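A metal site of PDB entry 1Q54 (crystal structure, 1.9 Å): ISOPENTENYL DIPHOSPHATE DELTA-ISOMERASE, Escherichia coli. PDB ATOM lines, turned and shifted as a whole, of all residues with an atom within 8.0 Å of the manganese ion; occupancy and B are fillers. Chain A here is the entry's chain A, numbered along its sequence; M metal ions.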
ATOM      1  N   VAL A   6      -2.797 -12.698  -7.070  1.00  0.00           N
ATOM      2  CA  VAL A   6      -3.236 -12.296  -8.401  1.00  0.00           C
ATOM      3  C   VAL A   6      -4.732 -12.618  -8.487  1.00  0.00           C
ATOM      4  O   VAL A   6      -5.224 -13.415  -7.685  1.00  0.00           O
ATOM      5  CB  VAL A   6      -2.481 -12.953  -9.561  1.00  0.00           C
ATOM      6  CG1 VAL A   6      -0.972 -12.858  -9.368  1.00  0.00           C
ATOM      7  CG2 VAL A   6      -2.888 -14.415  -9.724  1.00  0.00           C
ATOM      8  N   ILE A   7      -5.424 -12.020  -9.445  1.00  0.00           N
ATOM      9  CA  ILE A   7      -6.857 -12.225  -9.558  1.00  0.00           C
ATOM     10  C   ILE A   7      -7.220 -13.014 -10.807  1.00  0.00           C
ATOM     11  O   ILE A   7      -7.024 -12.494 -11.905  1.00  0.00           O
ATOM     12  CB  ILE A   7      -7.617 -10.879  -9.587  1.00  0.00           C
ATOM     13  CG1 ILE A   7      -7.399 -10.032  -8.333  1.00  0.00           C
ATOM     14  CG2 ILE A   7      -9.094 -11.142  -9.856  1.00  0.00           C
ATOM     15  CD1 ILE A   7      -7.957  -8.640  -8.420  1.00  0.00           C
ATOM     16  N   LYS A  21       0.679 -14.860  -5.122  1.00  0.00           N
ATOM     17  CA  LYS A  21       1.386 -14.390  -6.312  1.00  0.00           C
ATOM     18  C   LYS A  21       2.479 -15.355  -6.758  1.00  0.00           C
ATOM     19  O   LYS A  21       2.584 -15.683  -7.939  1.00  0.00           O
ATOM     20  CB  LYS A  21       1.972 -12.992  -6.098  1.00  0.00           C
ATOM     21  CG  LYS A  21       2.614 -12.409  -7.360  1.00  0.00           C
ATOM     22  CD  LYS A  21       2.880 -10.930  -7.206  1.00  0.00           C
ATOM     23  CE  LYS A  21       4.190 -10.676  -6.470  1.00  0.00           C
ATOM     24  NZ  LYS A  21       4.724  -9.306  -6.736  1.00  0.00           N
ATOM     25  N   ALA A  24       1.333 -18.517  -8.403  1.00  0.00           N
ATOM     26  CA  ALA A  24       0.454 -18.377  -9.556  1.00  0.00           C
ATOM     27  C   ALA A  24       1.209 -18.404 -10.879  1.00  0.00           C
ATOM     28  O   ALA A  24       0.640 -18.626 -11.949  1.00  0.00           O
ATOM     29  CB  ALA A  24      -0.352 -17.089  -9.466  1.00  0.00           C
ATOM     30  N   HIS A  25       2.508 -18.168 -10.830  1.00  0.00           N
ATOM     31  CA  HIS A  25       3.268 -18.125 -12.087  1.00  0.00           C
ATOM     32  C   HIS A  25       4.046 -19.426 -12.246  1.00  0.00           C
ATOM     33  O   HIS A  25       4.993 -19.724 -11.523  1.00  0.00           O
ATOM     34  CB  HIS A  25       4.165 -16.889 -12.113  1.00  0.00           C
ATOM     35  CG  HIS A  25       3.310 -15.645 -12.152  1.00  0.00           C
ATOM     36  ND1 HIS A  25       2.984 -14.923 -11.029  1.00  0.00           N
ATOM     37  CD2 HIS A  25       2.723 -15.031 -13.194  1.00  0.00           C
ATOM     38  CE1 HIS A  25       2.210 -13.899 -11.400  1.00  0.00           C
ATOM     39  NE2 HIS A  25       2.043 -13.939 -12.713  1.00  0.00           N
ATOM     40  N   THR A  29       0.595 -21.162 -16.087  1.00  0.00           N
ATOM     41  CA  THR A  29      -0.100 -20.011 -15.519  1.00  0.00           C
ATOM     42  C   THR A  29      -1.486 -19.777 -16.101  1.00  0.00           C
ATOM     43  O   THR A  29      -1.664 -19.740 -17.316  1.00  0.00           O
ATOM     44  CB  THR A  29       0.743 -18.734 -15.730  1.00  0.00           C
ATOM     45  OG1 THR A  29       1.988 -18.948 -15.066  1.00  0.00           O
ATOM     46  CG2 THR A  29       0.093 -17.505 -15.120  1.00  0.00           C
ATOM     47  N   ARG A  30      -2.470 -19.608 -15.217  1.00  0.00           N
ATOM     48  CA  ARG A  30      -3.846 -19.347 -15.620  1.00  0.00           C
ATOM     49  C   ARG A  30      -4.088 -17.856 -15.800  1.00  0.00           C
ATOM     50  O   ARG A  30      -3.422 -17.018 -15.222  1.00  0.00           O
ATOM     51  CB  ARG A  30      -4.844 -19.910 -14.596  1.00  0.00           C
ATOM     52  CG  ARG A  30      -4.309 -21.039 -13.753  1.00  0.00           C
ATOM     53  CD  ARG A  30      -5.216 -22.224 -13.592  1.00  0.00           C
ATOM     54  NE  ARG A  30      -6.574 -21.991 -13.183  1.00  0.00           N
ATOM     55  CZ  ARG A  30      -7.151 -22.347 -12.041  1.00  0.00           C
ATOM     56  NH1 ARG A  30      -6.478 -23.006 -11.093  1.00  0.00           N
ATOM     57  NH2 ARG A  30      -8.430 -22.054 -11.826  1.00  0.00           N
ATOM     58  N   LEU A  31      -5.072 -17.530 -16.624  1.00  0.00           N
ATOM     59  CA  LEU A  31      -5.377 -16.130 -16.916  1.00  0.00           C
ATOM     60  C   LEU A  31      -5.639 -15.334 -15.648  1.00  0.00           C
ATOM     61  O   LEU A  31      -6.513 -15.694 -14.844  1.00  0.00           O
ATOM     62  CB  LEU A  31      -6.578 -16.079 -17.855  1.00  0.00           C
ATOM     63  CG  LEU A  31      -7.045 -14.698 -18.328  1.00  0.00           C
ATOM     64  CD1 LEU A  31      -5.887 -13.956 -18.982  1.00  0.00           C
ATOM     65  CD2 LEU A  31      -8.214 -14.855 -19.288  1.00  0.00           C
ATOM     66  N   HIS A  32      -4.918 -14.227 -15.451  1.00  0.00           N
ATOM     67  CA  HIS A  32      -5.204 -13.382 -14.285  1.00  0.00           C
ATOM     68  C   HIS A  32      -5.102 -11.902 -14.653  1.00  0.00           C
ATOM     69  O   HIS A  32      -4.858 -11.533 -15.793  1.00  0.00           O
ATOM     70  CB  HIS A  32      -4.290 -13.742 -13.112  1.00  0.00           C
ATOM     71  CG  HIS A  32      -2.833 -13.709 -13.461  1.00  0.00           C
ATOM     72  ND1 HIS A  32      -2.179 -14.749 -14.058  1.00  0.00           N
ATOM     73  CD2 HIS A  32      -1.889 -12.760 -13.274  1.00  0.00           C
ATOM     74  CE1 HIS A  32      -0.896 -14.456 -14.241  1.00  0.00           C
ATOM     75  NE2 HIS A  32      -0.701 -13.242 -13.763  1.00  0.00           N
ATOM     76  N   LEU A  33      -5.314 -11.045 -13.666  1.00  0.00           N
ATOM     77  CA  LEU A  33      -5.333  -9.604 -13.890  1.00  0.00           C
ATOM     78  C   LEU A  33      -3.990  -8.946 -13.602  1.00  0.00           C
ATOM     79  O   LEU A  33      -3.302  -9.259 -12.623  1.00  0.00           O
ATOM     80  CB  LEU A  33      -6.401  -8.952 -13.007  1.00  0.00           C
ATOM     81  CG  LEU A  33      -6.790  -7.517 -13.373  1.00  0.00           C
ATOM     82  CD1 LEU A  33      -7.347  -7.429 -14.793  1.00  0.00           C
ATOM     83  CD2 LEU A  33      -7.807  -6.979 -12.359  1.00  0.00           C
ATOM     84  N   ALA A  34      -3.601  -8.022 -14.478  1.00  0.00           N
ATOM     85  CA  ALA A  34      -2.314  -7.346 -14.374  1.00  0.00           C
ATOM     86  C   ALA A  34      -2.373  -5.935 -14.953  1.00  0.00           C
ATOM     87  O   ALA A  34      -3.370  -5.513 -15.516  1.00  0.00           O
ATOM     88  CB  ALA A  34      -1.239  -8.151 -15.096  1.00  0.00           C
ATOM     89  N   PHE A  35      -1.258  -5.206 -14.815  1.00  0.00           N
ATOM     90  CA  PHE A  35      -1.174  -3.904 -15.451  1.00  0.00           C
ATOM     91  C   PHE A  35       0.228  -3.780 -16.057  1.00  0.00           C
ATOM     92  O   PHE A  35       1.133  -4.465 -15.591  1.00  0.00           O
ATOM     93  CB  PHE A  35      -1.412  -2.700 -14.541  1.00  0.00           C
ATOM     94  CG  PHE A  35      -0.334  -2.443 -13.493  1.00  0.00           C
ATOM     95  CD1 PHE A  35       0.762  -1.610 -13.670  1.00  0.00           C
ATOM     96  CD2 PHE A  35      -0.460  -3.079 -12.265  1.00  0.00           C
ATOM     97  CE1 PHE A  35       1.721  -1.432 -12.698  1.00  0.00           C
ATOM     98  CE2 PHE A  35       0.490  -2.914 -11.274  1.00  0.00           C
ATOM     99  CZ  PHE A  35       1.580  -2.090 -11.491  1.00  0.00           C
ATOM    100  N   ARG A  51      14.577  -6.437 -15.421  1.00  0.00           N
ATOM    101  CA  ARG A  51      14.042  -7.144 -14.248  1.00  0.00           C
ATOM    102  C   ARG A  51      15.148  -7.855 -13.469  1.00  0.00           C
ATOM    103  O   ARG A  51      16.123  -8.368 -14.022  1.00  0.00           O
ATOM    104  CB  ARG A  51      12.966  -8.127 -14.704  1.00  0.00           C
ATOM    105  CG  ARG A  51      11.808  -7.476 -15.432  1.00  0.00           C
ATOM    106  CD  ARG A  51      10.971  -8.524 -16.144  1.00  0.00           C
ATOM    107  NE  ARG A  51      10.335  -9.486 -15.265  1.00  0.00           N
ATOM    108  CZ  ARG A  51       9.261  -9.288 -14.507  1.00  0.00           C
ATOM    109  NH1 ARG A  51       8.669  -8.091 -14.496  1.00  0.00           N
ATOM    110  NH2 ARG A  51       8.783 -10.268 -13.747  1.00  0.00           N
ATOM    111  N   ALA A  57       9.336 -14.640 -13.336  1.00  0.00           N
ATOM    112  CA  ALA A  57       9.076 -14.592 -14.772  1.00  0.00           C
ATOM    113  C   ALA A  57       9.958 -13.538 -15.431  1.00  0.00           C
ATOM    114  O   ALA A  57      10.124 -12.449 -14.893  1.00  0.00           O
ATOM    115  CB  ALA A  57       7.605 -14.320 -15.040  1.00  0.00           C
ATOM    116  N   TRP A  58      10.501 -13.868 -16.581  1.00  0.00           N
ATOM    117  CA  TRP A  58      11.441 -13.014 -17.327  1.00  0.00           C
ATOM    118  C   TRP A  58      12.473 -12.338 -16.437  1.00  0.00           C
ATOM    119  O   TRP A  58      12.695 -11.132 -16.497  1.00  0.00           O
ATOM    120  CB  TRP A  58      10.655 -11.972 -18.151  1.00  0.00           C
ATOM    121  CG  TRP A  58      10.067 -12.652 -19.353  1.00  0.00           C
ATOM    122  CD1 TRP A  58      10.670 -12.757 -20.586  1.00  0.00           C
ATOM    123  CD2 TRP A  58       8.802 -13.308 -19.459  1.00  0.00           C
ATOM    124  NE1 TRP A  58       9.843 -13.437 -21.439  1.00  0.00           N
ATOM    125  CE2 TRP A  58       8.693 -13.788 -20.777  1.00  0.00           C
ATOM    126  CE3 TRP A  58       7.737 -13.549 -18.584  1.00  0.00           C
ATOM    127  CZ2 TRP A  58       7.569 -14.487 -21.239  1.00  0.00           C
ATOM    128  CZ3 TRP A  58       6.627 -14.240 -19.029  1.00  0.00           C
ATOM    129  CH2 TRP A  58       6.551 -14.696 -20.342  1.00  0.00           C
ATOM    130  N   GLY A  68       2.630  -5.037 -12.993  1.00  0.00           N
ATOM    131  CA  GLY A  68       2.240  -5.687 -11.760  1.00  0.00           C
ATOM    132  C   GLY A  68       0.846  -6.278 -11.823  1.00  0.00           C
ATOM    133  O   GLY A  68       0.254  -6.430 -12.892  1.00  0.00           O
ATOM    134  N   HIS A  69       0.350  -6.592 -10.636  1.00  0.00           N
ATOM    135  CA  HIS A  69      -0.870  -7.328 -10.399  1.00  0.00           C
ATOM    136  C   HIS A  69      -1.786  -6.604  -9.408  1.00  0.00           C
ATOM    137  O   HIS A  69      -1.501  -6.586  -8.206  1.00  0.00           O
ATOM    138  CB  HIS A  69      -0.537  -8.713  -9.845  1.00  0.00           C
ATOM    139  CG  HIS A  69       0.226  -9.592 -10.762  1.00  0.00           C
ATOM    140  ND1 HIS A  69       1.601  -9.747 -10.689  1.00  0.00           N
ATOM    141  CD2 HIS A  69      -0.165 -10.384 -11.788  1.00  0.00           C
ATOM    142  CE1 HIS A  69       2.003 -10.588 -11.624  1.00  0.00           C
ATOM    143  NE2 HIS A  69       0.952 -10.998 -12.321  1.00  0.00           N
ATOM    144  N   VAL A 113       5.249 -19.157 -17.529  1.00  0.00           N
ATOM    145  CA  VAL A 113       4.253 -18.488 -18.373  1.00  0.00           C
ATOM    146  C   VAL A 113       3.629 -17.290 -17.670  1.00  0.00           C
ATOM    147  O   VAL A 113       3.364 -17.303 -16.464  1.00  0.00           O
ATOM    148  CB  VAL A 113       3.123 -19.446 -18.788  1.00  0.00           C
ATOM    149  CG1 VAL A 113       1.983 -18.682 -19.474  1.00  0.00           C
ATOM    150  CG2 VAL A 113       3.625 -20.564 -19.696  1.00  0.00           C
ATOM    151  N   GLU A 114       3.378 -16.228 -18.433  1.00  0.00           N
ATOM    152  CA  GLU A 114       2.509 -15.143 -18.008  1.00  0.00           C
ATOM    153  C   GLU A 114       1.279 -15.187 -18.915  1.00  0.00           C
ATOM    154  O   GLU A 114       1.381 -15.443 -20.111  1.00  0.00           O
ATOM    155  CB  GLU A 114       3.160 -13.765 -18.035  1.00  0.00           C
ATOM    156  CG  GLU A 114       3.880 -13.408 -16.741  1.00  0.00           C
ATOM    157  CD  GLU A 114       2.911 -12.941 -15.662  1.00  0.00           C
ATOM    158  OE1 GLU A 114       3.318 -12.156 -14.773  1.00  0.00           O
ATOM    159  OE2 GLU A 114       1.766 -13.429 -15.592  1.00  0.00           O
ATOM    160  N   ASN A 115       0.125 -14.948 -18.302  1.00  0.00           N
ATOM    161  CA  ASN A 115      -1.149 -15.097 -19.008  1.00  0.00           C
ATOM    162  C   ASN A 115      -2.145 -14.113 -18.429  1.00  0.00           C
ATOM    163  O   ASN A 115      -2.721 -14.310 -17.371  1.00  0.00           O
ATOM    164  CB  ASN A 115      -1.615 -16.543 -18.873  1.00  0.00           C
ATOM    165  CG  ASN A 115      -2.796 -16.867 -19.765  1.00  0.00           C
ATOM    166  OD1 ASN A 115      -3.198 -16.018 -20.561  1.00  0.00           O
ATOM    167  ND2 ASN A 115      -3.330 -18.065 -19.602  1.00  0.00           N
ATOM    168  N   GLU A 116      -2.300 -12.983 -19.117  1.00  0.00           N
ATOM    169  CA  GLU A 116      -2.885 -11.824 -18.481  1.00  0.00           C
ATOM    170  C   GLU A 116      -3.756 -10.978 -19.404  1.00  0.00           C
ATOM    171  O   GLU A 116      -3.492 -10.830 -20.590  1.00  0.00           O
ATOM    172  CB  GLU A 116      -1.770 -10.923 -17.942  1.00  0.00           C
ATOM    173  CG  GLU A 116      -1.059 -11.496 -16.725  1.00  0.00           C
ATOM    174  CD  GLU A 116       0.235 -10.798 -16.371  1.00  0.00           C
ATOM    175  OE1 GLU A 116       0.726  -9.993 -17.199  1.00  0.00           O
ATOM    176  OE2 GLU A 116       0.766 -11.015 -15.256  1.00  0.00           O
ATOM    177  N   TRP A 161       6.358  -8.782 -23.771  1.00  0.00           N
ATOM    178  CA  TRP A 161       5.276  -7.930 -23.278  1.00  0.00           C
ATOM    179  C   TRP A 161       5.440  -6.490 -23.692  1.00  0.00           C
ATOM    180  O   TRP A 161       4.529  -5.790 -24.131  1.00  0.00           O
ATOM    181  CB  TRP A 161       5.184  -8.037 -21.742  1.00  0.00           C
ATOM    182  CG  TRP A 161       4.686  -9.408 -21.412  1.00  0.00           C
ATOM    183  CD1 TRP A 161       5.465 -10.515 -21.193  1.00  0.00           C
ATOM    184  CD2 TRP A 161       3.333  -9.847 -21.254  1.00  0.00           C
ATOM    185  NE1 TRP A 161       4.682 -11.603 -20.921  1.00  0.00           N
ATOM    186  CE2 TRP A 161       3.359 -11.214 -20.955  1.00  0.00           C
ATOM    187  CE3 TRP A 161       2.098  -9.186 -21.344  1.00  0.00           C
ATOM    188  CZ2 TRP A 161       2.197 -11.961 -20.733  1.00  0.00           C
ATOM    189  CZ3 TRP A 161       0.946  -9.931 -21.136  1.00  0.00           C
ATOM    190  CH2 TRP A 161       1.012 -11.298 -20.833  1.00  0.00           C
HETATM  191 MN    MN M   1       1.201 -12.464 -13.712  1.00  0.00          MN
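A ring nitrogen (ND1) of His 25 lies within hydrogen-bond range of the backbone carbonyl oxygen (O) of Lys 21 (3.2 Å).
The backbone carbonyl oxygen (O) of Asn 115 sits at hydrogen-bond distance from the backbone NH (N) of His 32 (2.9 Å).
ND1 of His 32 lies within hydrogen-bond range of O of Arg 30, 2.8 Å away.
Within 4 Å of the manganese ion: His 25, His 32, His 69, Glu 114 and Glu 116.
The nearest printed residue that does not touch the manganese ion is Val 6 (4.9 Å).
The manganese ion is bound by NE2 of His 25, at 2.0 Å.
NE2 of His 69 binds the manganese ion, at 2.0 Å.
NE2 of His 32 binds the manganese ion, at 2.1 Å.
The manganese ion is bound by OE2 of Glu 116 (2.2 Å).
The manganese ion is bound by OE2 of Glu 114, at 2.2 Å.
The side-chain carboxylate (OE1) of Glu 114 binds the manganese ion (2.4 Å).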
